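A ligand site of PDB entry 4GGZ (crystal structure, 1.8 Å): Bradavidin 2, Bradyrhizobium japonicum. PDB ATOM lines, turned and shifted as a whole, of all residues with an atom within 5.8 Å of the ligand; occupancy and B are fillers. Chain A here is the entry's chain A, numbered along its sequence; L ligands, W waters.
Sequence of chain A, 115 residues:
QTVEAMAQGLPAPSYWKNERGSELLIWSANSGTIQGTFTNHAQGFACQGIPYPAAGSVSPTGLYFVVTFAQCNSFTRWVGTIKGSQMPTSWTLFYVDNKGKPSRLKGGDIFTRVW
Arg 20 touches the ligand (CD to N1, 3.7 Å). Phe 38 touches the ligand (CZ to O3, 3.6 Å). CB of Ala 42 touches N2 of the ligand (3.3 Å). Phe 45 touches the ligand (CB to O1, 3.7 Å). CG of Phe 69 touches C2 of the ligand, at 3.6 Å. Cys 72 touches the ligand. Trp 78 touches the ligand (CZ2 to S1, 3.5 Å). Trp 91 touches the ligand. CD1 of Leu 93 touches O2 of the ligand, at 3.98 Å. 16 residues have an atom within 4 Å of the ligand: Asn 18, Arg 20, Ser 22, Phe 38, Asn 40, Ala 42, Phe 45, Ala 46, Phe 69, Cys 72, Ser 74, Thr 76, Trp 78, Trp 91, Leu 93 and Asp 109.
OD1 of Asp 109 is in salt-bridge range of NE of Arg 20 (2.7 Å). NH2 of Arg 20 lies within hydrogen-bond range of O of Gly 108, 2.8 Å away. SG of Cys 47 forms a disulfide with SG of Cys 72. The side-chain amide oxygen of Asn 40 lies within hydrogen-bond range of the backbone NH of Ala 42, 2.8 Å away. The side-chain amide oxygen of Asn 18 lies within hydrogen-bond range of the backbone NH of Arg 20, 2.9 Å away. The indole nitrogen (NE1) of Trp 91 is in hydrogen-bond range of the backbone carbonyl oxygen (O) of Gly 108 (3.0 Å). The side-chain amide oxygen of Asn 40 is in hydrogen-bond range of the side-chain hydroxyl of Ser 22 (3.1 Å). The side-chain amide nitrogen of Asn 18 lies within hydrogen-bond range of the side-chain carboxylate of Asp 109 (3.2 Å).
An oxygen (O2) of the ligand lies within hydrogen-bond range of the side-chain hydroxyl (OG) of Ser 74, 2.7 Å away. OD2 of Asp 109 is in hydrogen-bond range of N1 of the ligand, at 2.9 Å. OG of Ser 22 lies within hydrogen-bond range of O3 of the ligand (2.7 Å). The side-chain amide oxygen (OD1) of Asn 40 is in hydrogen-bond range of a nitrogen (N2) of the ligand (2.9 Å). The side-chain amide nitrogen of Asn 18 lies within hydrogen-bond range of an oxygen (O3) of the ligand (2.8 Å). OG1 of Thr 76 lies close to S1 of the ligand, at 3.4 Å. An oxygen (O1) of the ligand lies within hydrogen-bond range of the backbone NH (N) of Ala 46, 3.2 Å away.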
ATOM      1  N   ASN A  18     -17.347   8.917   9.286  1.00  0.00           N
ATOM      2  CA  ASN A  18     -18.032   7.996   8.366  1.00  0.00           C
ATOM      3  C   ASN A  18     -17.228   7.859   7.085  1.00  0.00           C
ATOM      4  O   ASN A  18     -16.153   8.453   6.984  1.00  0.00           O
ATOM      5  CB  ASN A  18     -19.498   8.329   8.099  1.00  0.00           C
ATOM      6  CG  ASN A  18     -19.695   9.625   7.350  1.00  0.00           C
ATOM      7  OD1 ASN A  18     -18.805  10.078   6.663  1.00  0.00           O
ATOM      8  ND2 ASN A  18     -20.917  10.229   7.505  1.00  0.00           N
ATOM      9  N   ARG A  20     -17.615   9.006   4.253  1.00  0.00           N
ATOM     10  CA  ARG A  20     -17.580  10.201   3.413  1.00  0.00           C
ATOM     11  C   ARG A  20     -16.589  11.230   3.961  1.00  0.00           C
ATOM     12  O   ARG A  20     -16.290  12.238   3.306  1.00  0.00           O
ATOM     13  CB  ARG A  20     -18.987  10.813   3.378  1.00  0.00           C
ATOM     14  CG  ARG A  20     -20.076   9.824   3.033  1.00  0.00           C
ATOM     15  CD  ARG A  20     -21.424  10.483   3.045  1.00  0.00           C
ATOM     16  NE  ARG A  20     -22.469   9.482   2.913  1.00  0.00           N
ATOM     17  CZ  ARG A  20     -23.234   9.358   1.845  1.00  0.00           C
ATOM     18  NH1 ARG A  20     -23.056  10.187   0.824  1.00  0.00           N
ATOM     19  NH2 ARG A  20     -24.165   8.412   1.793  1.00  0.00           N
ATOM     20  N   SER A  22     -17.058  12.525   7.149  1.00  0.00           N
ATOM     21  CA  SER A  22     -17.751  13.402   8.122  1.00  0.00           C
ATOM     22  C   SER A  22     -17.455  12.965   9.551  1.00  0.00           C
ATOM     23  O   SER A  22     -17.157  11.786   9.762  1.00  0.00           O
ATOM     24  CB  SER A  22     -19.255  13.419   7.871  1.00  0.00           C
ATOM     25  OG  SER A  22     -19.567  14.076   6.616  1.00  0.00           O
ATOM     26  N   PHE A  38     -21.739  17.369  15.058  1.00  0.00           N
ATOM     27  CA  PHE A  38     -21.479  16.708  13.761  1.00  0.00           C
ATOM     28  C   PHE A  38     -20.889  17.750  12.837  1.00  0.00           C
ATOM     29  O   PHE A  38     -21.353  18.882  12.807  1.00  0.00           O
ATOM     30  CB  PHE A  38     -22.798  16.196  13.160  1.00  0.00           C
ATOM     31  CG  PHE A  38     -22.646  15.556  11.793  1.00  0.00           C
ATOM     32  CD1 PHE A  38     -22.323  14.214  11.684  1.00  0.00           C
ATOM     33  CD2 PHE A  38     -22.845  16.308  10.639  1.00  0.00           C
ATOM     34  CE1 PHE A  38     -22.183  13.609  10.409  1.00  0.00           C
ATOM     35  CE2 PHE A  38     -22.682  15.704   9.358  1.00  0.00           C
ATOM     36  CZ  PHE A  38     -22.389  14.353   9.289  1.00  0.00           C
ATOM     37  N   ASN A  40     -20.014  18.051   8.659  1.00  0.00           N
ATOM     38  CA  ASN A  40     -20.034  17.410   7.316  1.00  0.00           C
ATOM     39  C   ASN A  40     -18.713  17.599   6.609  1.00  0.00           C
ATOM     40  O   ASN A  40     -18.170  18.704   6.610  1.00  0.00           O
ATOM     41  CB  ASN A  40     -21.168  18.021   6.480  1.00  0.00           C
ATOM     42  CG  ASN A  40     -21.263  17.398   5.095  1.00  0.00           C
ATOM     43  OD1 ASN A  40     -21.166  16.182   4.960  1.00  0.00           O
ATOM     44  ND2 ASN A  40     -21.438  18.230   4.086  1.00  0.00           N
ATOM     45  N   HIS A  41     -18.264  16.556   5.909  1.00  0.00           N
ATOM     46  CA  HIS A  41     -17.163  16.689   4.977  1.00  0.00           C
ATOM     47  C   HIS A  41     -17.491  15.906   3.726  1.00  0.00           C
ATOM     48  O   HIS A  41     -16.587  15.626   2.922  1.00  0.00           O
ATOM     49  CB  HIS A  41     -15.867  16.150   5.626  1.00  0.00           C
ATOM     50  CG  HIS A  41     -15.351  17.017   6.723  1.00  0.00           C
ATOM     51  ND1 HIS A  41     -14.942  18.326   6.503  1.00  0.00           N
ATOM     52  CD2 HIS A  41     -15.195  16.794   8.046  1.00  0.00           C
ATOM     53  CE1 HIS A  41     -14.558  18.853   7.659  1.00  0.00           C
ATOM     54  NE2 HIS A  41     -14.702  17.947   8.611  1.00  0.00           N
ATOM     55  N   ALA A  42     -18.777  15.582   3.559  1.00  0.00           N
ATOM     56  CA  ALA A  42     -19.230  14.731   2.460  1.00  0.00           C
ATOM     57  C   ALA A  42     -19.213  15.423   1.115  1.00  0.00           C
ATOM     58  O   ALA A  42     -19.786  16.468   0.920  1.00  0.00           O
ATOM     59  CB  ALA A  42     -20.630  14.164   2.768  1.00  0.00           C
ATOM     60  N   GLY A  44     -20.505  16.367  -2.338  1.00  0.00           N
ATOM     61  CA  GLY A  44     -21.818  16.431  -2.947  1.00  0.00           C
ATOM     62  C   GLY A  44     -22.843  17.090  -2.040  1.00  0.00           C
ATOM     63  O   GLY A  44     -24.024  17.118  -2.396  1.00  0.00           O
ATOM     64  N   PHE A  45     -22.391  17.596  -0.889  1.00  0.00           N
ATOM     65  CA  PHE A  45     -23.250  18.268   0.109  1.00  0.00           C
ATOM     66  C   PHE A  45     -22.609  19.600   0.543  1.00  0.00           C
ATOM     67  O   PHE A  45     -21.409  19.809   0.382  1.00  0.00           O
ATOM     68  CB  PHE A  45     -23.463  17.382   1.319  1.00  0.00           C
ATOM     69  CG  PHE A  45     -24.137  16.055   0.989  1.00  0.00           C
ATOM     70  CD1 PHE A  45     -23.387  14.951   0.599  1.00  0.00           C
ATOM     71  CD2 PHE A  45     -25.529  15.922   1.080  1.00  0.00           C
ATOM     72  CE1 PHE A  45     -24.024  13.674   0.309  1.00  0.00           C
ATOM     73  CE2 PHE A  45     -26.191  14.689   0.804  1.00  0.00           C
ATOM     74  CZ  PHE A  45     -25.405  13.549   0.396  1.00  0.00           C
ATOM     75  N   ALA A  46     -23.418  20.479   1.134  1.00  0.00           N
ATOM     76  CA  ALA A  46     -22.949  21.804   1.538  1.00  0.00           C
ATOM     77  C   ALA A  46     -22.671  21.852   3.056  1.00  0.00           C
ATOM     78  O   ALA A  46     -22.630  20.826   3.731  1.00  0.00           O
ATOM     79  CB  ALA A  46     -23.994  22.815   1.161  1.00  0.00           C
ATOM     80  N   CYS A  47     -22.451  23.051   3.590  1.00  0.00           N
ATOM     81  CA  CYS A  47     -22.149  23.222   5.022  1.00  0.00           C
ATOM     82  C   CYS A  47     -20.897  22.416   5.450  1.00  0.00           C
ATOM     83  O   CYS A  47     -20.806  21.911   6.561  1.00  0.00           O
ATOM     84  CB  CYS A  47     -23.357  22.822   5.865  1.00  0.00           C
ATOM     85  SG  CYS A  47     -24.755  24.005   5.866  1.00  0.00           S
ATOM     86  N   PHE A  69     -28.738  21.638   9.896  1.00  0.00           N
ATOM     87  CA  PHE A  69     -27.740  22.407   9.187  1.00  0.00           C
ATOM     88  C   PHE A  69     -28.347  23.761   8.860  1.00  0.00           C
ATOM     89  O   PHE A  69     -28.913  23.973   7.780  1.00  0.00           O
ATOM     90  CB  PHE A  69     -27.305  21.662   7.907  1.00  0.00           C
ATOM     91  CG  PHE A  69     -26.762  20.305   8.164  1.00  0.00           C
ATOM     92  CD1 PHE A  69     -27.596  19.194   8.070  1.00  0.00           C
ATOM     93  CD2 PHE A  69     -25.420  20.118   8.467  1.00  0.00           C
ATOM     94  CE1 PHE A  69     -27.120  17.899   8.315  1.00  0.00           C
ATOM     95  CE2 PHE A  69     -24.903  18.828   8.708  1.00  0.00           C
ATOM     96  CZ  PHE A  69     -25.763  17.724   8.630  1.00  0.00           C
ATOM     97  N   CYS A  72     -27.904  25.709   5.622  1.00  0.00           N
ATOM     98  CA  CYS A  72     -28.343  24.980   4.415  1.00  0.00           C
ATOM     99  C   CYS A  72     -29.878  24.761   4.391  1.00  0.00           C
ATOM    100  O   CYS A  72     -30.413  24.137   3.475  1.00  0.00           O
ATOM    101  CB  CYS A  72     -27.574  23.657   4.333  1.00  0.00           C
ATOM    102  SG  CYS A  72     -25.752  23.856   4.010  1.00  0.00           S
ATOM    103  N   SER A  74     -31.667  22.813   6.078  1.00  0.00           N
ATOM    104  CA  SER A  74     -31.893  21.366   6.007  1.00  0.00           C
ATOM    105  C   SER A  74     -31.614  20.715   7.367  1.00  0.00           C
ATOM    106  O   SER A  74     -30.988  21.345   8.229  1.00  0.00           O
ATOM    107  CB  SER A  74     -31.009  20.776   4.902  1.00  0.00           C
ATOM    108  OG  SER A  74     -29.637  20.802   5.259  1.00  0.00           O
ATOM    109  N   THR A  76     -30.844  16.401   8.925  1.00  0.00           N
ATOM    110  CA  THR A  76     -30.757  14.973   8.632  1.00  0.00           C
ATOM    111  C   THR A  76     -31.061  14.139   9.863  1.00  0.00           C
ATOM    112  O   THR A  76     -30.656  14.514  10.948  1.00  0.00           O
ATOM    113  CB  THR A  76     -29.350  14.667   8.111  1.00  0.00           C
ATOM    114  OG1 THR A  76     -29.155  15.430   6.914  1.00  0.00           O
ATOM    115  CG2 THR A  76     -29.171  13.170   7.814  1.00  0.00           C
ATOM    116  N   TRP A  78     -30.384  10.312  11.203  1.00  0.00           N
ATOM    117  CA  TRP A  78     -29.791   8.978  11.076  1.00  0.00           C
ATOM    118  C   TRP A  78     -30.458   7.972  12.009  1.00  0.00           C
ATOM    119  O   TRP A  78     -30.822   8.311  13.132  1.00  0.00           O
ATOM    120  CB  TRP A  78     -28.295   8.948  11.441  1.00  0.00           C
ATOM    121  CG  TRP A  78     -27.367   9.647  10.492  1.00  0.00           C
ATOM    122  CD1 TRP A  78     -26.563   9.027   9.493  1.00  0.00           C
ATOM    123  CD2 TRP A  78     -27.098  11.042  10.406  1.00  0.00           C
ATOM    124  NE1 TRP A  78     -25.810  10.006   8.852  1.00  0.00           N
ATOM    125  CE2 TRP A  78     -26.127  11.239   9.379  1.00  0.00           C
ATOM    126  CE3 TRP A  78     -27.563  12.177  11.135  1.00  0.00           C
ATOM    127  CZ2 TRP A  78     -25.606  12.515   9.048  1.00  0.00           C
ATOM    128  CZ3 TRP A  78     -27.060  13.491  10.757  1.00  0.00           C
ATOM    129  CH2 TRP A  78     -26.081  13.624   9.731  1.00  0.00           C
ATOM    130  N   TRP A  91     -30.030   7.289   6.594  1.00  0.00           N
ATOM    131  CA  TRP A  91     -30.397   8.652   6.916  1.00  0.00           C
ATOM    132  C   TRP A  91     -31.373   9.211   5.890  1.00  0.00           C
ATOM    133  O   TRP A  91     -31.407   8.776   4.724  1.00  0.00           O
ATOM    134  CB  TRP A  91     -29.152   9.578   7.031  1.00  0.00           C
ATOM    135  CG  TRP A  91     -28.222   9.562   5.793  1.00  0.00           C
ATOM    136  CD1 TRP A  91     -27.091   8.816   5.641  1.00  0.00           C
ATOM    137  CD2 TRP A  91     -28.393  10.297   4.545  1.00  0.00           C
ATOM    138  NE1 TRP A  91     -26.542   9.017   4.378  1.00  0.00           N
ATOM    139  CE2 TRP A  91     -27.318   9.911   3.690  1.00  0.00           C
ATOM    140  CE3 TRP A  91     -29.357  11.206   4.063  1.00  0.00           C
ATOM    141  CZ2 TRP A  91     -27.169  10.435   2.399  1.00  0.00           C
ATOM    142  CZ3 TRP A  91     -29.194  11.738   2.797  1.00  0.00           C
ATOM    143  CH2 TRP A  91     -28.105  11.328   1.958  1.00  0.00           C
ATOM    144  N   LEU A  93     -32.410  13.221   4.628  1.00  0.00           N
ATOM    145  CA  LEU A  93     -32.050  14.638   4.686  1.00  0.00           C
ATOM    146  C   LEU A  93     -33.276  15.377   4.208  1.00  0.00           C
ATOM    147  O   LEU A  93     -33.709  15.171   3.080  1.00  0.00           O
ATOM    148  CB  LEU A  93     -30.822  14.927   3.793  1.00  0.00           C
ATOM    149  CG  LEU A  93     -30.454  16.379   3.454  1.00  0.00           C
ATOM    150  CD1 LEU A  93     -29.888  17.101   4.626  1.00  0.00           C
ATOM    151  CD2 LEU A  93     -29.406  16.476   2.293  1.00  0.00           C
ATOM    152  N   TYR A  95     -34.934  18.894   3.338  1.00  0.00           N
ATOM    153  CA  TYR A  95     -34.486  20.256   3.040  1.00  0.00           C
ATOM    154  C   TYR A  95     -35.607  21.126   2.466  1.00  0.00           C
ATOM    155  O   TYR A  95     -36.537  20.602   1.859  1.00  0.00           O
ATOM    156  CB  TYR A  95     -33.244  20.246   2.140  1.00  0.00           C
ATOM    157  CG  TYR A  95     -33.404  19.671   0.747  1.00  0.00           C
ATOM    158  CD1 TYR A  95     -33.434  18.276   0.535  1.00  0.00           C
ATOM    159  CD2 TYR A  95     -33.538  20.515  -0.361  1.00  0.00           C
ATOM    160  CE1 TYR A  95     -33.552  17.738  -0.786  1.00  0.00           C
ATOM    161  CE2 TYR A  95     -33.641  19.988  -1.671  1.00  0.00           C
ATOM    162  CZ  TYR A  95     -33.657  18.619  -1.874  1.00  0.00           C
ATOM    163  OH  TYR A  95     -33.760  18.119  -3.160  1.00  0.00           O
ATOM    164  N   GLY A 108     -27.179   5.941   2.975  1.00  0.00           N
ATOM    165  CA  GLY A 108     -26.592   5.236   4.090  1.00  0.00           C
ATOM    166  C   GLY A 108     -25.313   5.874   4.589  1.00  0.00           C
ATOM    167  O   GLY A 108     -24.697   6.725   3.909  1.00  0.00           O
ATOM    168  N   ASP A 109     -24.915   5.490   5.809  1.00  0.00           N
ATOM    169  CA  ASP A 109     -23.617   5.865   6.327  1.00  0.00           C
ATOM    170  C   ASP A 109     -23.150   4.785   7.274  1.00  0.00           C
ATOM    171  O   ASP A 109     -23.939   4.221   7.996  1.00  0.00           O
ATOM    172  CB  ASP A 109     -23.711   7.145   7.137  1.00  0.00           C
ATOM    173  CG  ASP A 109     -23.394   8.392   6.337  1.00  0.00           C
ATOM    174  OD1 ASP A 109     -22.576   8.347   5.390  1.00  0.00           O
ATOM    175  OD2 ASP A 109     -23.953   9.441   6.701  1.00  0.00           O
ATOM    176  N   PHE A 111     -20.513   4.737  10.293  1.00  0.00           N
ATOM    177  CA  PHE A 111     -19.511   5.390  11.107  1.00  0.00           C
ATOM    178  C   PHE A 111     -18.604   4.385  11.817  1.00  0.00           C
ATOM    179  O   PHE A 111     -19.064   3.337  12.282  1.00  0.00           O
ATOM    180  CB  PHE A 111     -20.202   6.222  12.207  1.00  0.00           C
ATOM    181  CG  PHE A 111     -20.999   7.382  11.670  1.00  0.00           C
ATOM    182  CD1 PHE A 111     -22.282   7.181  11.170  1.00  0.00           C
ATOM    183  CD2 PHE A 111     -20.472   8.683  11.674  1.00  0.00           C
ATOM    184  CE1 PHE A 111     -23.060   8.271  10.671  1.00  0.00           C
ATOM    185  CE2 PHE A 111     -21.243   9.767  11.181  1.00  0.00           C
ATOM    186  CZ  PHE A 111     -22.518   9.556  10.663  1.00  0.00           C
HETATM  187  C1  LIG L   1     -26.941  19.970   3.205  1.00  0.00           C
HETATM  188  O1  LIG L   1     -26.292  19.647   2.157  1.00  0.00           O
HETATM  189  O2  LIG L   1     -28.149  20.340   3.093  1.00  0.00           O
HETATM  190  C2  LIG L   1     -26.322  19.957   4.589  1.00  0.00           C
HETATM  191  C3  LIG L   1     -25.235  18.886   4.770  1.00  0.00           C
HETATM  192  C4  LIG L   1     -25.843  17.480   4.640  1.00  0.00           C
HETATM  193  C5  LIG L   1     -24.782  16.385   4.827  1.00  0.00           C
HETATM  194  C6  LIG L   1     -25.413  14.983   4.690  1.00  0.00           C
HETATM  195  S1  LIG L   1     -26.033  14.387   6.151  1.00  0.00           S
HETATM  196  C7  LIG L   1     -26.200  12.751   5.367  1.00  0.00           C
HETATM  197  C8  LIG L   1     -24.920  12.552   4.549  1.00  0.00           C
HETATM  198  N1  LIG L   1     -23.857  11.998   5.356  1.00  0.00           N
HETATM  199  C9  LIG L   1     -22.865  12.884   5.495  1.00  0.00           C
HETATM  200  O3  LIG L   1     -21.733  12.600   6.198  1.00  0.00           O
HETATM  201  N2  LIG L   1     -23.104  14.024   4.888  1.00  0.00           N
HETATM  202  C10 LIG L   1     -24.406  13.928   4.213  1.00  0.00           C
HETATM  203  O   HOH W   1     -26.637  19.800  -0.376  1.00  0.00           O
